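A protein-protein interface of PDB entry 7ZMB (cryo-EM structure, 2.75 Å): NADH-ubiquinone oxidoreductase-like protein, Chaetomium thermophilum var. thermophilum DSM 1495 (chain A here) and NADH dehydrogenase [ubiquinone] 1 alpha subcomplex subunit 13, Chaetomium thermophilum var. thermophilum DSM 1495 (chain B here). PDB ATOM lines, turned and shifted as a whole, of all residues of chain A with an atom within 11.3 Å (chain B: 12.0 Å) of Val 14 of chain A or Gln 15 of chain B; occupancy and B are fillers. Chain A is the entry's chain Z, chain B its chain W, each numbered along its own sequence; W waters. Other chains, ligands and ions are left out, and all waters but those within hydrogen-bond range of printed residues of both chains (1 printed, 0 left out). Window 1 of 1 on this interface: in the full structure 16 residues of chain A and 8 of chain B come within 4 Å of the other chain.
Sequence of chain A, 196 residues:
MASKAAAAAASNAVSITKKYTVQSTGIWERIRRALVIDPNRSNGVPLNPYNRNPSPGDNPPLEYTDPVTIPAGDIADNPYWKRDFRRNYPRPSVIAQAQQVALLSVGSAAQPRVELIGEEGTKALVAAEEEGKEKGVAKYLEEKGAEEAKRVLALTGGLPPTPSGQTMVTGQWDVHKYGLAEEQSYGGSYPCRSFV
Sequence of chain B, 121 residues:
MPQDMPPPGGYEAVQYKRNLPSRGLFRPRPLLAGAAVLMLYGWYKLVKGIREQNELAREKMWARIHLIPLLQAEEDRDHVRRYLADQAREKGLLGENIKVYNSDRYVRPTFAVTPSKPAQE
The side-chain amino group (NZ) of Lys 19 of chain A is in hydrogen-bond range of the side-chain amide oxygen (OE1) of Gln 15 of chain B (3.4 Å).
NZ of Lys 17 of chain B lies within salt-bridge range of OE1 of Glu 183 of chain A (3.7 Å).
NH2 of Arg 41 of chain A sits at hydrogen-bond distance from O of Asn 19 of chain B (3.3 Å).
O of Lys 17 of chain B is in hydrogen-bond range of NE2 of Gln 15 of chain B (3.4 Å).
The backbone carbonyl oxygen (O) of Val 14 of chain A is in hydrogen-bond range of the side-chain amide nitrogen (ND2) of Asn 40 of chain A (3.4 Å).
The side-chain amino group (NZ) of Lys 19 of chain A is in hydrogen-bond range of the backbone carbonyl oxygen (O) of Asn 40 of chain A (2.5 Å).
The side-chain carboxylate (OD1) of Asp 38 of chain A lies within hydrogen-bond range of the backbone NH (N) of Asn 40 of chain A, at 3.1 Å.
CG of Gln 15 of chain B touches O of Asn 12 of chain A, at 3.5 Å.
Asn 12 of chain A touches Lys 17 of chain B.
CB of Ala 13 of chain A touches ND2 of Asn 19 of chain B (3.5 Å).
CG2 of Val 14 of chain A touches CB of Gln 15 of chain B (3.8 Å).
Asp 38 of chain A touches Asn 19 of chain B.
CG of Pro 21 of chain B touches OD2 of Asp 38 of chain A, 3.1 Å away.
Ser 185 of chain A touches Arg 18 of chain B.
Val 14 of chain A touches just one residue of chain B: Gln 15 (3.8 Å).
Gln 15 of chain B touches just these residues of chain A: Asn 12, Val 14 and Lys 19.
Ser 15 of chain A touches none of the printed residues of chain B.
No residue of chain B comes within 4 Å of Ile 16 of chain A.
No residue of chain B comes within 4 Å of Asn 40 of chain A.
No residue of chain A comes within 4 Å of Ala 13 of chain B.
No residue of chain A comes within 4 Å of Val 14 of chain B.
Printed residues of chain A within 4 Å of Arg 18 of chain B: Ser 185 (3.7 Å).
Printed residues of chain A within 4 Å of Pro 21 of chain B: Asp 38.
The nearest residue of chain B that does not touch Val 14 of chain A is Val 14 of chain B (4.4 Å).
The nearest residue of chain A that does not touch Gln 15 of chain B is Ala 13 of chain A (4.2 Å).
Of the 11 printed residues of chain B, 5 touch a printed residue of chain A.
Hydrophobic or aromatic side chains of chain B within 4 Å of the printed part of chain A: Pro 21.
Printed residues of chain A that touch a printed residue of chain B: Asn 12, Ala 13, Val 14, Lys 19, Asp 38, Arg 41, Glu 183 and Ser 185.
Hydrophobic or aromatic side chains of chain A within 4 Å of the printed part of chain B: Ala 13 and Val 14.
Along chain A the printed residues that touch a printed residue of chain B span positions 12 to 185.
Water W1 lies within hydrogen-bond range of the guanidinium group (NE) of Arg 41 of chain A (2.4 Å) and the backbone carbonyl oxygen (O) of Asn 19 of chain B (2.6 Å).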
ATOM      1  N   SER A  11      15.218 -32.177   2.451  1.00  0.00           N
ATOM      2  CA  SER A  11      16.295 -31.197   2.371  1.00  0.00           C
ATOM      3  C   SER A  11      15.751 -29.821   2.013  1.00  0.00           C
ATOM      4  O   SER A  11      14.657 -29.700   1.464  1.00  0.00           O
ATOM      5  CB  SER A  11      17.340 -31.627   1.341  1.00  0.00           C
ATOM      6  OG  SER A  11      16.918 -31.303   0.026  1.00  0.00           O
ATOM      7  N   ASN A  12      16.525 -28.783   2.328  1.00  0.00           N
ATOM      8  CA  ASN A  12      16.146 -27.409   1.997  1.00  0.00           C
ATOM      9  C   ASN A  12      16.600 -27.080   0.574  1.00  0.00           C
ATOM     10  O   ASN A  12      17.376 -26.158   0.323  1.00  0.00           O
ATOM     11  CB  ASN A  12      16.732 -26.432   3.005  1.00  0.00           C
ATOM     12  CG  ASN A  12      16.448 -26.826   4.434  1.00  0.00           C
ATOM     13  OD1 ASN A  12      15.327 -27.192   4.780  1.00  0.00           O
ATOM     14  ND2 ASN A  12      17.471 -26.758   5.278  1.00  0.00           N
ATOM     15  N   ALA A  13      16.093 -27.861  -0.368  1.00  0.00           N
ATOM     16  CA  ALA A  13      16.281 -27.591  -1.782  1.00  0.00           C
ATOM     17  C   ALA A  13      14.938 -27.246  -2.402  1.00  0.00           C
ATOM     18  O   ALA A  13      13.931 -27.899  -2.120  1.00  0.00           O
ATOM     19  CB  ALA A  13      16.897 -28.785  -2.507  1.00  0.00           C
ATOM     20  N   VAL A  14      14.922 -26.209  -3.228  1.00  0.00           N
ATOM     21  CA  VAL A  14      13.766 -25.947  -4.068  1.00  0.00           C
ATOM     22  C   VAL A  14      13.980 -26.685  -5.382  1.00  0.00           C
ATOM     23  O   VAL A  14      15.093 -27.081  -5.723  1.00  0.00           O
ATOM     24  CB  VAL A  14      13.522 -24.434  -4.297  1.00  0.00           C
ATOM     25  CG1 VAL A  14      13.514 -23.681  -2.977  1.00  0.00           C
ATOM     26  CG2 VAL A  14      14.519 -23.856  -5.242  1.00  0.00           C
ATOM     27  N   SER A  15      12.899 -26.890  -6.124  1.00  0.00           N
ATOM     28  CA  SER A  15      12.975 -27.684  -7.338  1.00  0.00           C
ATOM     29  C   SER A  15      13.715 -26.942  -8.443  1.00  0.00           C
ATOM     30  O   SER A  15      13.654 -25.715  -8.552  1.00  0.00           O
ATOM     31  CB  SER A  15      11.583 -28.057  -7.823  1.00  0.00           C
ATOM     32  OG  SER A  15      11.606 -28.436  -9.188  1.00  0.00           O
ATOM     33  N   ILE A  16      14.410 -27.713  -9.282  1.00  0.00           N
ATOM     34  CA  ILE A  16      15.090 -27.151 -10.442  1.00  0.00           C
ATOM     35  C   ILE A  16      14.114 -26.441 -11.370  1.00  0.00           C
ATOM     36  O   ILE A  16      14.489 -25.491 -12.061  1.00  0.00           O
ATOM     37  CB  ILE A  16      15.855 -28.267 -11.181  1.00  0.00           C
ATOM     38  CG1 ILE A  16      16.770 -27.689 -12.256  1.00  0.00           C
ATOM     39  CG2 ILE A  16      14.898 -29.258 -11.792  1.00  0.00           C
ATOM     40  CD1 ILE A  16      17.699 -26.669 -11.744  1.00  0.00           C
ATOM     41  N   THR A  17      12.853 -26.854 -11.362  1.00  0.00           N
ATOM     42  CA  THR A  17      11.861 -26.382 -12.308  1.00  0.00           C
ATOM     43  C   THR A  17      11.381 -24.969 -11.982  1.00  0.00           C
ATOM     44  O   THR A  17      10.609 -24.387 -12.752  1.00  0.00           O
ATOM     45  CB  THR A  17      10.721 -27.401 -12.323  1.00  0.00           C
ATOM     46  OG1 THR A  17      11.253 -28.677 -12.673  1.00  0.00           O
ATOM     47  CG2 THR A  17       9.730 -27.077 -13.383  1.00  0.00           C
ATOM     48  N   LYS A  18      11.850 -24.385 -10.879  1.00  0.00           N
ATOM     49  CA  LYS A  18      11.513 -23.013 -10.529  1.00  0.00           C
ATOM     50  C   LYS A  18      12.707 -22.060 -10.569  1.00  0.00           C
ATOM     51  O   LYS A  18      12.566 -20.900 -10.175  1.00  0.00           O
ATOM     52  CB  LYS A  18      10.875 -22.964  -9.140  1.00  0.00           C
ATOM     53  CG  LYS A  18       9.561 -23.684  -9.021  1.00  0.00           C
ATOM     54  CD  LYS A  18       8.983 -23.502  -7.620  1.00  0.00           C
ATOM     55  CE  LYS A  18       9.768 -24.254  -6.558  1.00  0.00           C
ATOM     56  NZ  LYS A  18       9.678 -25.719  -6.724  1.00  0.00           N
ATOM     57  N   LYS A  19      13.870 -22.502 -11.050  1.00  0.00           N
ATOM     58  CA  LYS A  19      15.127 -21.815 -10.782  1.00  0.00           C
ATOM     59  C   LYS A  19      15.619 -20.920 -11.918  1.00  0.00           C
ATOM     60  O   LYS A  19      16.743 -20.416 -11.838  1.00  0.00           O
ATOM     61  CB  LYS A  19      16.203 -22.833 -10.411  1.00  0.00           C
ATOM     62  CG  LYS A  19      16.045 -23.364  -9.003  1.00  0.00           C
ATOM     63  CD  LYS A  19      17.080 -24.402  -8.649  1.00  0.00           C
ATOM     64  CE  LYS A  19      17.293 -24.440  -7.150  1.00  0.00           C
ATOM     65  NZ  LYS A  19      18.198 -25.521  -6.715  1.00  0.00           N
ATOM     66  N   TYR A  20      14.811 -20.693 -12.952  1.00  0.00           N
ATOM     67  CA  TYR A  20      15.085 -19.687 -13.993  1.00  0.00           C
ATOM     68  C   TYR A  20      16.440 -19.877 -14.665  1.00  0.00           C
ATOM     69  O   TYR A  20      17.153 -18.916 -14.951  1.00  0.00           O
ATOM     70  CB  TYR A  20      14.960 -18.260 -13.453  1.00  0.00           C
ATOM     71  CG  TYR A  20      13.537 -17.823 -13.288  1.00  0.00           C
ATOM     72  CD1 TYR A  20      12.827 -17.307 -14.355  1.00  0.00           C
ATOM     73  CD2 TYR A  20      12.894 -17.944 -12.073  1.00  0.00           C
ATOM     74  CE1 TYR A  20      11.528 -16.926 -14.217  1.00  0.00           C
ATOM     75  CE2 TYR A  20      11.589 -17.557 -11.927  1.00  0.00           C
ATOM     76  CZ  TYR A  20      10.909 -17.052 -13.002  1.00  0.00           C
ATOM     77  OH  TYR A  20       9.600 -16.664 -12.854  1.00  0.00           O
ATOM     78  N   THR A  21      16.788 -21.121 -14.948  1.00  0.00           N
ATOM     79  CA  THR A  21      17.981 -21.431 -15.715  1.00  0.00           C
ATOM     80  C   THR A  21      17.592 -22.337 -16.873  1.00  0.00           C
ATOM     81  O   THR A  21      16.508 -22.918 -16.891  1.00  0.00           O
ATOM     82  CB  THR A  21      19.081 -22.085 -14.846  1.00  0.00           C
ATOM     83  OG1 THR A  21      18.568 -23.247 -14.183  1.00  0.00           O
ATOM     84  CG2 THR A  21      19.613 -21.112 -13.824  1.00  0.00           C
ATOM     85  N   GLN A  23      17.338 -25.534 -19.055  1.00  0.00           N
ATOM     86  CA  GLN A  23      17.087 -26.879 -18.575  1.00  0.00           C
ATOM     87  C   GLN A  23      17.607 -27.907 -19.568  1.00  0.00           C
ATOM     88  O   GLN A  23      17.772 -27.635 -20.757  1.00  0.00           O
ATOM     89  CB  GLN A  23      15.591 -27.110 -18.356  1.00  0.00           C
ATOM     90  CG  GLN A  23      14.899 -26.030 -17.562  1.00  0.00           C
ATOM     91  CD  GLN A  23      15.021 -26.210 -16.068  1.00  0.00           C
ATOM     92  OE1 GLN A  23      15.694 -25.443 -15.392  1.00  0.00           O
ATOM     93  NE2 GLN A  23      14.351 -27.223 -15.545  1.00  0.00           N
ATOM     94  N   ARG A  32      21.109 -36.761 -16.840  1.00  0.00           N
ATOM     95  CA  ARG A  32      21.701 -35.860 -15.862  1.00  0.00           C
ATOM     96  C   ARG A  32      21.159 -36.119 -14.461  1.00  0.00           C
ATOM     97  O   ARG A  32      21.919 -36.079 -13.490  1.00  0.00           O
ATOM     98  CB  ARG A  32      21.504 -34.402 -16.287  1.00  0.00           C
ATOM     99  CG  ARG A  32      20.136 -33.825 -16.079  1.00  0.00           C
ATOM    100  CD  ARG A  32      20.204 -32.325 -16.003  1.00  0.00           C
ATOM    101  NE  ARG A  32      20.511 -31.865 -14.661  1.00  0.00           N
ATOM    102  CZ  ARG A  32      19.600 -31.642 -13.726  1.00  0.00           C
ATOM    103  NH1 ARG A  32      18.316 -31.835 -13.980  1.00  0.00           N
ATOM    104  NH2 ARG A  32      19.980 -31.225 -12.531  1.00  0.00           N
ATOM    105  N   ARG A  33      19.863 -36.422 -14.328  1.00  0.00           N
ATOM    106  CA  ARG A  33      19.344 -36.753 -13.005  1.00  0.00           C
ATOM    107  C   ARG A  33      19.878 -38.081 -12.497  1.00  0.00           C
ATOM    108  O   ARG A  33      19.891 -38.305 -11.284  1.00  0.00           O
ATOM    109  CB  ARG A  33      17.818 -36.761 -13.008  1.00  0.00           C
ATOM    110  CG  ARG A  33      17.222 -35.392 -13.239  1.00  0.00           C
ATOM    111  CD  ARG A  33      15.716 -35.423 -13.264  1.00  0.00           C
ATOM    112  NE  ARG A  33      15.155 -35.771 -11.966  1.00  0.00           N
ATOM    113  CZ  ARG A  33      13.867 -36.024 -11.759  1.00  0.00           C
ATOM    114  NH1 ARG A  33      13.440 -36.333 -10.543  1.00  0.00           N
ATOM    115  NH2 ARG A  33      13.010 -35.965 -12.768  1.00  0.00           N
ATOM    116  N   ILE A  37      24.938 -35.042  -8.432  1.00  0.00           N
ATOM    117  CA  ILE A  37      24.812 -35.159  -6.988  1.00  0.00           C
ATOM    118  C   ILE A  37      23.482 -34.598  -6.515  1.00  0.00           C
ATOM    119  O   ILE A  37      22.848 -35.157  -5.622  1.00  0.00           O
ATOM    120  CB  ILE A  37      26.013 -34.473  -6.306  1.00  0.00           C
ATOM    121  CG1 ILE A  37      27.234 -35.377  -6.380  1.00  0.00           C
ATOM    122  CG2 ILE A  37      25.709 -34.128  -4.867  1.00  0.00           C
ATOM    123  CD1 ILE A  37      28.530 -34.632  -6.441  1.00  0.00           C
ATOM    124  N   ASP A  38      23.033 -33.514  -7.126  1.00  0.00           N
ATOM    125  CA  ASP A  38      21.724 -32.950  -6.841  1.00  0.00           C
ATOM    126  C   ASP A  38      21.048 -32.531  -8.138  1.00  0.00           C
ATOM    127  O   ASP A  38      21.434 -31.522  -8.741  1.00  0.00           O
ATOM    128  CB  ASP A  38      21.833 -31.753  -5.897  1.00  0.00           C
ATOM    129  CG  ASP A  38      20.573 -31.535  -5.100  1.00  0.00           C
ATOM    130  OD1 ASP A  38      19.567 -31.071  -5.673  1.00  0.00           O
ATOM    131  OD2 ASP A  38      20.582 -31.831  -3.895  1.00  0.00           O
ATOM    132  N   PRO A  39      20.031 -33.266  -8.592  1.00  0.00           N
ATOM    133  CA  PRO A  39      19.326 -32.875  -9.821  1.00  0.00           C
ATOM    134  C   PRO A  39      18.524 -31.594  -9.690  1.00  0.00           C
ATOM    135  O   PRO A  39      18.023 -31.100 -10.703  1.00  0.00           O
ATOM    136  CB  PRO A  39      18.418 -34.074 -10.095  1.00  0.00           C
ATOM    137  CG  PRO A  39      18.240 -34.709  -8.771  1.00  0.00           C
ATOM    138  CD  PRO A  39      19.519 -34.529  -8.046  1.00  0.00           C
ATOM    139  N   ASN A  40      18.375 -31.050  -8.488  1.00  0.00           N
ATOM    140  CA  ASN A  40      17.731 -29.761  -8.319  1.00  0.00           C
ATOM    141  C   ASN A  40      18.708 -28.593  -8.372  1.00  0.00           C
ATOM    142  O   ASN A  40      18.263 -27.445  -8.375  1.00  0.00           O
ATOM    143  CB  ASN A  40      16.954 -29.731  -7.000  1.00  0.00           C
ATOM    144  CG  ASN A  40      15.511 -30.165  -7.166  1.00  0.00           C
ATOM    145  OD1 ASN A  40      14.993 -30.225  -8.279  1.00  0.00           O
ATOM    146  ND2 ASN A  40      14.854 -30.463  -6.059  1.00  0.00           N
ATOM    147  N   ARG A  41      20.018 -28.850  -8.411  1.00  0.00           N
ATOM    148  CA  ARG A  41      20.978 -27.786  -8.665  1.00  0.00           C
ATOM    149  C   ARG A  41      20.893 -27.319 -10.107  1.00  0.00           C
ATOM    150  O   ARG A  41      20.755 -28.125 -11.030  1.00  0.00           O
ATOM    151  CB  ARG A  41      22.407 -28.242  -8.375  1.00  0.00           C
ATOM    152  CG  ARG A  41      22.781 -28.265  -6.923  1.00  0.00           C
ATOM    153  CD  ARG A  41      24.205 -28.731  -6.725  1.00  0.00           C
ATOM    154  NE  ARG A  41      24.515 -28.809  -5.306  1.00  0.00           N
ATOM    155  CZ  ARG A  41      25.652 -29.259  -4.794  1.00  0.00           C
ATOM    156  NH1 ARG A  41      26.628 -29.685  -5.582  1.00  0.00           N
ATOM    157  NH2 ARG A  41      25.809 -29.278  -3.481  1.00  0.00           N
ATOM    158  N   SER A  42      21.014 -26.013 -10.298  1.00  0.00           N
ATOM    159  CA  SER A  42      20.971 -25.388 -11.609  1.00  0.00           C
ATOM    160  C   SER A  42      22.374 -25.225 -12.181  1.00  0.00           C
ATOM    161  O   SER A  42      23.373 -25.227 -11.461  1.00  0.00           O
ATOM    162  CB  SER A  42      20.275 -24.031 -11.522  1.00  0.00           C
ATOM    163  OG  SER A  42      20.718 -23.289 -10.400  1.00  0.00           O
ATOM    164  N   ASN A  43      22.436 -25.087 -13.498  1.00  0.00           N
ATOM    165  CA  ASN A  43      23.702 -24.923 -14.193  1.00  0.00           C
ATOM    166  C   ASN A  43      24.190 -23.481 -14.220  1.00  0.00           C
ATOM    167  O   ASN A  43      25.335 -23.243 -14.605  1.00  0.00           O
ATOM    168  CB  ASN A  43      23.587 -25.461 -15.625  1.00  0.00           C
ATOM    169  CG  ASN A  43      22.492 -24.782 -16.419  1.00  0.00           C
ATOM    170  OD1 ASN A  43      21.832 -23.865 -15.940  1.00  0.00           O
ATOM    171  ND2 ASN A  43      22.294 -25.235 -17.651  1.00  0.00           N
ATOM    172  N   GLY A  44      23.355 -22.522 -13.830  1.00  0.00           N
ATOM    173  CA  GLY A  44      23.743 -21.129 -13.797  1.00  0.00           C
ATOM    174  C   GLY A  44      23.602 -20.369 -15.095  1.00  0.00           C
ATOM    175  O   GLY A  44      24.047 -19.222 -15.167  1.00  0.00           O
ATOM    176  N   GLU A 183      17.143 -21.750  13.856  1.00  0.00           N
ATOM    177  CA  GLU A 183      17.742 -22.727  12.964  1.00  0.00           C
ATOM    178  C   GLU A 183      19.230 -22.428  12.856  1.00  0.00           C
ATOM    179  O   GLU A 183      19.618 -21.284  12.596  1.00  0.00           O
ATOM    180  CB  GLU A 183      17.092 -22.687  11.581  1.00  0.00           C
ATOM    181  CG  GLU A 183      17.653 -23.716  10.600  1.00  0.00           C
ATOM    182  CD  GLU A 183      18.711 -23.146   9.665  1.00  0.00           C
ATOM    183  OE1 GLU A 183      19.409 -23.943   9.004  1.00  0.00           O
ATOM    184  OE2 GLU A 183      18.845 -21.905   9.587  1.00  0.00           O
ATOM    185  N   SER A 185      22.449 -23.114  10.732  1.00  0.00           N
ATOM    186  CA  SER A 185      22.678 -23.578   9.369  1.00  0.00           C
ATOM    187  C   SER A 185      23.714 -24.687   9.312  1.00  0.00           C
ATOM    188  O   SER A 185      23.559 -25.644   8.548  1.00  0.00           O
ATOM    189  CB  SER A 185      23.091 -22.422   8.478  1.00  0.00           C
ATOM    190  OG  SER A 185      23.347 -22.879   7.165  1.00  0.00           O
ATOM    191  N   TYR B  11       7.424 -11.881  -4.718  1.00  0.00           N
ATOM    192  CA  TYR B  11       8.164 -12.981  -5.314  1.00  0.00           C
ATOM    193  C   TYR B  11       8.131 -14.210  -4.415  1.00  0.00           C
ATOM    194  O   TYR B  11       8.022 -14.117  -3.194  1.00  0.00           O
ATOM    195  CB  TYR B  11       9.615 -12.582  -5.576  1.00  0.00           C
ATOM    196  CG  TYR B  11       9.790 -11.462  -6.559  1.00  0.00           C
ATOM    197  CD1 TYR B  11       9.633 -11.675  -7.918  1.00  0.00           C
ATOM    198  CD2 TYR B  11      10.121 -10.183  -6.131  1.00  0.00           C
ATOM    199  CE1 TYR B  11       9.802 -10.646  -8.824  1.00  0.00           C
ATOM    200  CE2 TYR B  11      10.281  -9.155  -7.024  1.00  0.00           C
ATOM    201  CZ  TYR B  11      10.127  -9.392  -8.367  1.00  0.00           C
ATOM    202  OH  TYR B  11      10.290  -8.359  -9.249  1.00  0.00           O
ATOM    203  N   GLU B  12       8.220 -15.373  -5.046  1.00  0.00           N
ATOM    204  CA  GLU B  12       8.304 -16.630  -4.326  1.00  0.00           C
ATOM    205  C   GLU B  12       9.690 -16.808  -3.729  1.00  0.00           C
ATOM    206  O   GLU B  12      10.677 -16.257  -4.221  1.00  0.00           O
ATOM    207  CB  GLU B  12       7.974 -17.798  -5.249  1.00  0.00           C
ATOM    208  CG  GLU B  12       7.588 -19.047  -4.510  1.00  0.00           C
ATOM    209  CD  GLU B  12       6.551 -18.783  -3.437  1.00  0.00           C
ATOM    210  OE1 GLU B  12       5.464 -18.265  -3.771  1.00  0.00           O
ATOM    211  OE2 GLU B  12       6.830 -19.079  -2.257  1.00  0.00           O
ATOM    212  N   ALA B  13       9.754 -17.604  -2.665  1.00  0.00           N
ATOM    213  CA  ALA B  13      10.985 -17.785  -1.911  1.00  0.00           C
ATOM    214  C   ALA B  13      12.088 -18.374  -2.781  1.00  0.00           C
ATOM    215  O   ALA B  13      11.834 -19.087  -3.755  1.00  0.00           O
ATOM    216  CB  ALA B  13      10.736 -18.692  -0.714  1.00  0.00           C
ATOM    217  N   VAL B  14      13.325 -18.050  -2.430  1.00  0.00           N
ATOM    218  CA  VAL B  14      14.479 -18.612  -3.085  1.00  0.00           C
ATOM    219  C   VAL B  14      15.117 -19.642  -2.161  1.00  0.00           C
ATOM    220  O   VAL B  14      14.701 -19.832  -1.021  1.00  0.00           O
ATOM    221  CB  VAL B  14      15.492 -17.522  -3.514  1.00  0.00           C
ATOM    222  CG1 VAL B  14      14.889 -16.626  -4.585  1.00  0.00           C
ATOM    223  CG2 VAL B  14      15.943 -16.709  -2.322  1.00  0.00           C
ATOM    224  N   GLN B  15      16.124 -20.339  -2.671  1.00  0.00           N
ATOM    225  CA  GLN B  15      16.845 -21.360  -1.930  1.00  0.00           C
ATOM    226  C   GLN B  15      18.129 -20.748  -1.380  1.00  0.00           C
ATOM    227  O   GLN B  15      18.988 -20.317  -2.152  1.00  0.00           O
ATOM    228  CB  GLN B  15      17.140 -22.553  -2.838  1.00  0.00           C
ATOM    229  CG  GLN B  15      17.816 -23.719  -2.167  1.00  0.00           C
ATOM    230  CD  GLN B  15      19.216 -23.959  -2.681  1.00  0.00           C
ATOM    231  OE1 GLN B  15      19.444 -24.010  -3.881  1.00  0.00           O
ATOM    232  NE2 GLN B  15      20.167 -24.099  -1.770  1.00  0.00           N
ATOM    233  N   TYR B  16      18.255 -20.688  -0.058  1.00  0.00           N
ATOM    234  CA  TYR B  16      19.469 -20.105   0.505  1.00  0.00           C
ATOM    235  C   TYR B  16      20.079 -21.002   1.576  1.00  0.00           C
ATOM    236  O   TYR B  16      21.292 -20.970   1.787  1.00  0.00           O
ATOM    237  CB  TYR B  16      19.196 -18.698   1.058  1.00  0.00           C
ATOM    238  CG  TYR B  16      18.244 -18.618   2.228  1.00  0.00           C
ATOM    239  CD1 TYR B  16      18.691 -18.842   3.528  1.00  0.00           C
ATOM    240  CD2 TYR B  16      16.904 -18.327   2.041  1.00  0.00           C
ATOM    241  CE1 TYR B  16      17.835 -18.764   4.595  1.00  0.00           C
ATOM    242  CE2 TYR B  16      16.038 -18.258   3.107  1.00  0.00           C
ATOM    243  CZ  TYR B  16      16.510 -18.477   4.380  1.00  0.00           C
ATOM    244  OH  TYR B  16      15.650 -18.406   5.445  1.00  0.00           O
ATOM    245  N   LYS B  17      19.258 -21.809   2.246  1.00  0.00           N
ATOM    246  CA  LYS B  17      19.753 -22.726   3.266  1.00  0.00           C
ATOM    247  C   LYS B  17      20.771 -23.687   2.670  1.00  0.00           C
ATOM    248  O   LYS B  17      20.595 -24.191   1.560  1.00  0.00           O
ATOM    249  CB  LYS B  17      18.605 -23.534   3.874  1.00  0.00           C
ATOM    250  CG  LYS B  17      17.478 -22.751   4.507  1.00  0.00           C
ATOM    251  CD  LYS B  17      17.603 -22.664   6.009  1.00  0.00           C
ATOM    252  CE  LYS B  17      17.075 -21.344   6.517  1.00  0.00           C
ATOM    253  NZ  LYS B  17      17.226 -21.166   7.985  1.00  0.00           N
ATOM    254  N   ARG B  18      21.808 -23.968   3.470  1.00  0.00           N
ATOM    255  CA  ARG B  18      22.877 -24.902   3.053  1.00  0.00           C
ATOM    256  C   ARG B  18      22.254 -26.186   2.531  1.00  0.00           C
ATOM    257  O   ARG B  18      21.373 -26.746   3.217  1.00  0.00           O
ATOM    258  CB  ARG B  18      23.827 -25.150   4.223  1.00  0.00           C
ATOM    259  CG  ARG B  18      25.269 -25.408   3.824  1.00  0.00           C
ATOM    260  CD  ARG B  18      26.160 -25.423   5.046  1.00  0.00           C
ATOM    261  NE  ARG B  18      27.462 -25.985   4.730  1.00  0.00           N
ATOM    262  CZ  ARG B  18      27.769 -27.267   4.844  1.00  0.00           C
ATOM    263  NH1 ARG B  18      28.979 -27.688   4.525  1.00  0.00           N
ATOM    264  NH2 ARG B  18      26.865 -28.128   5.274  1.00  0.00           N
ATOM    265  N   ASN B  19      22.723 -26.649   1.385  1.00  0.00           N
ATOM    266  CA  ASN B  19      22.183 -27.849   0.742  1.00  0.00           C
ATOM    267  C   ASN B  19      23.324 -28.673   0.137  1.00  0.00           C
ATOM    268  O   ASN B  19      23.721 -28.466  -1.013  1.00  0.00           O
ATOM    269  CB  ASN B  19      21.133 -27.457  -0.293  1.00  0.00           C
ATOM    270  CG  ASN B  19      20.694 -28.618  -1.158  1.00  0.00           C
ATOM    271  OD1 ASN B  19      20.610 -29.752  -0.701  1.00  0.00           O
ATOM    272  ND2 ASN B  19      20.403 -28.335  -2.415  1.00  0.00           N
ATOM    273  N   LEU B  20      23.852 -29.614   0.919  1.00  0.00           N
ATOM    274  CA  LEU B  20      24.922 -30.519   0.495  1.00  0.00           C
ATOM    275  C   LEU B  20      24.528 -31.936   0.885  1.00  0.00           C
ATOM    276  O   LEU B  20      25.034 -32.484   1.872  1.00  0.00           O
ATOM    277  CB  LEU B  20      26.263 -30.134   1.121  1.00  0.00           C
ATOM    278  CG  LEU B  20      27.028 -28.909   0.613  1.00  0.00           C
ATOM    279  CD1 LEU B  20      26.464 -27.616   1.171  1.00  0.00           C
ATOM    280  CD2 LEU B  20      28.486 -29.043   0.960  1.00  0.00           C
ATOM    281  N   PRO B  21      23.631 -32.567   0.126  1.00  0.00           N
ATOM    282  CA  PRO B  21      23.010 -33.821   0.575  1.00  0.00           C
ATOM    283  C   PRO B  21      23.905 -35.030   0.336  1.00  0.00           C
ATOM    284  O   PRO B  21      24.478 -35.196  -0.741  1.00  0.00           O
ATOM    285  CB  PRO B  21      21.730 -33.893  -0.262  1.00  0.00           C
ATOM    286  CG  PRO B  21      22.079 -33.154  -1.508  1.00  0.00           C
ATOM    287  CD  PRO B  21      23.077 -32.100  -1.156  1.00  0.00           C
HETATM  288  O   HOH W   1      22.965 -28.911  -3.466  1.00  0.00           O
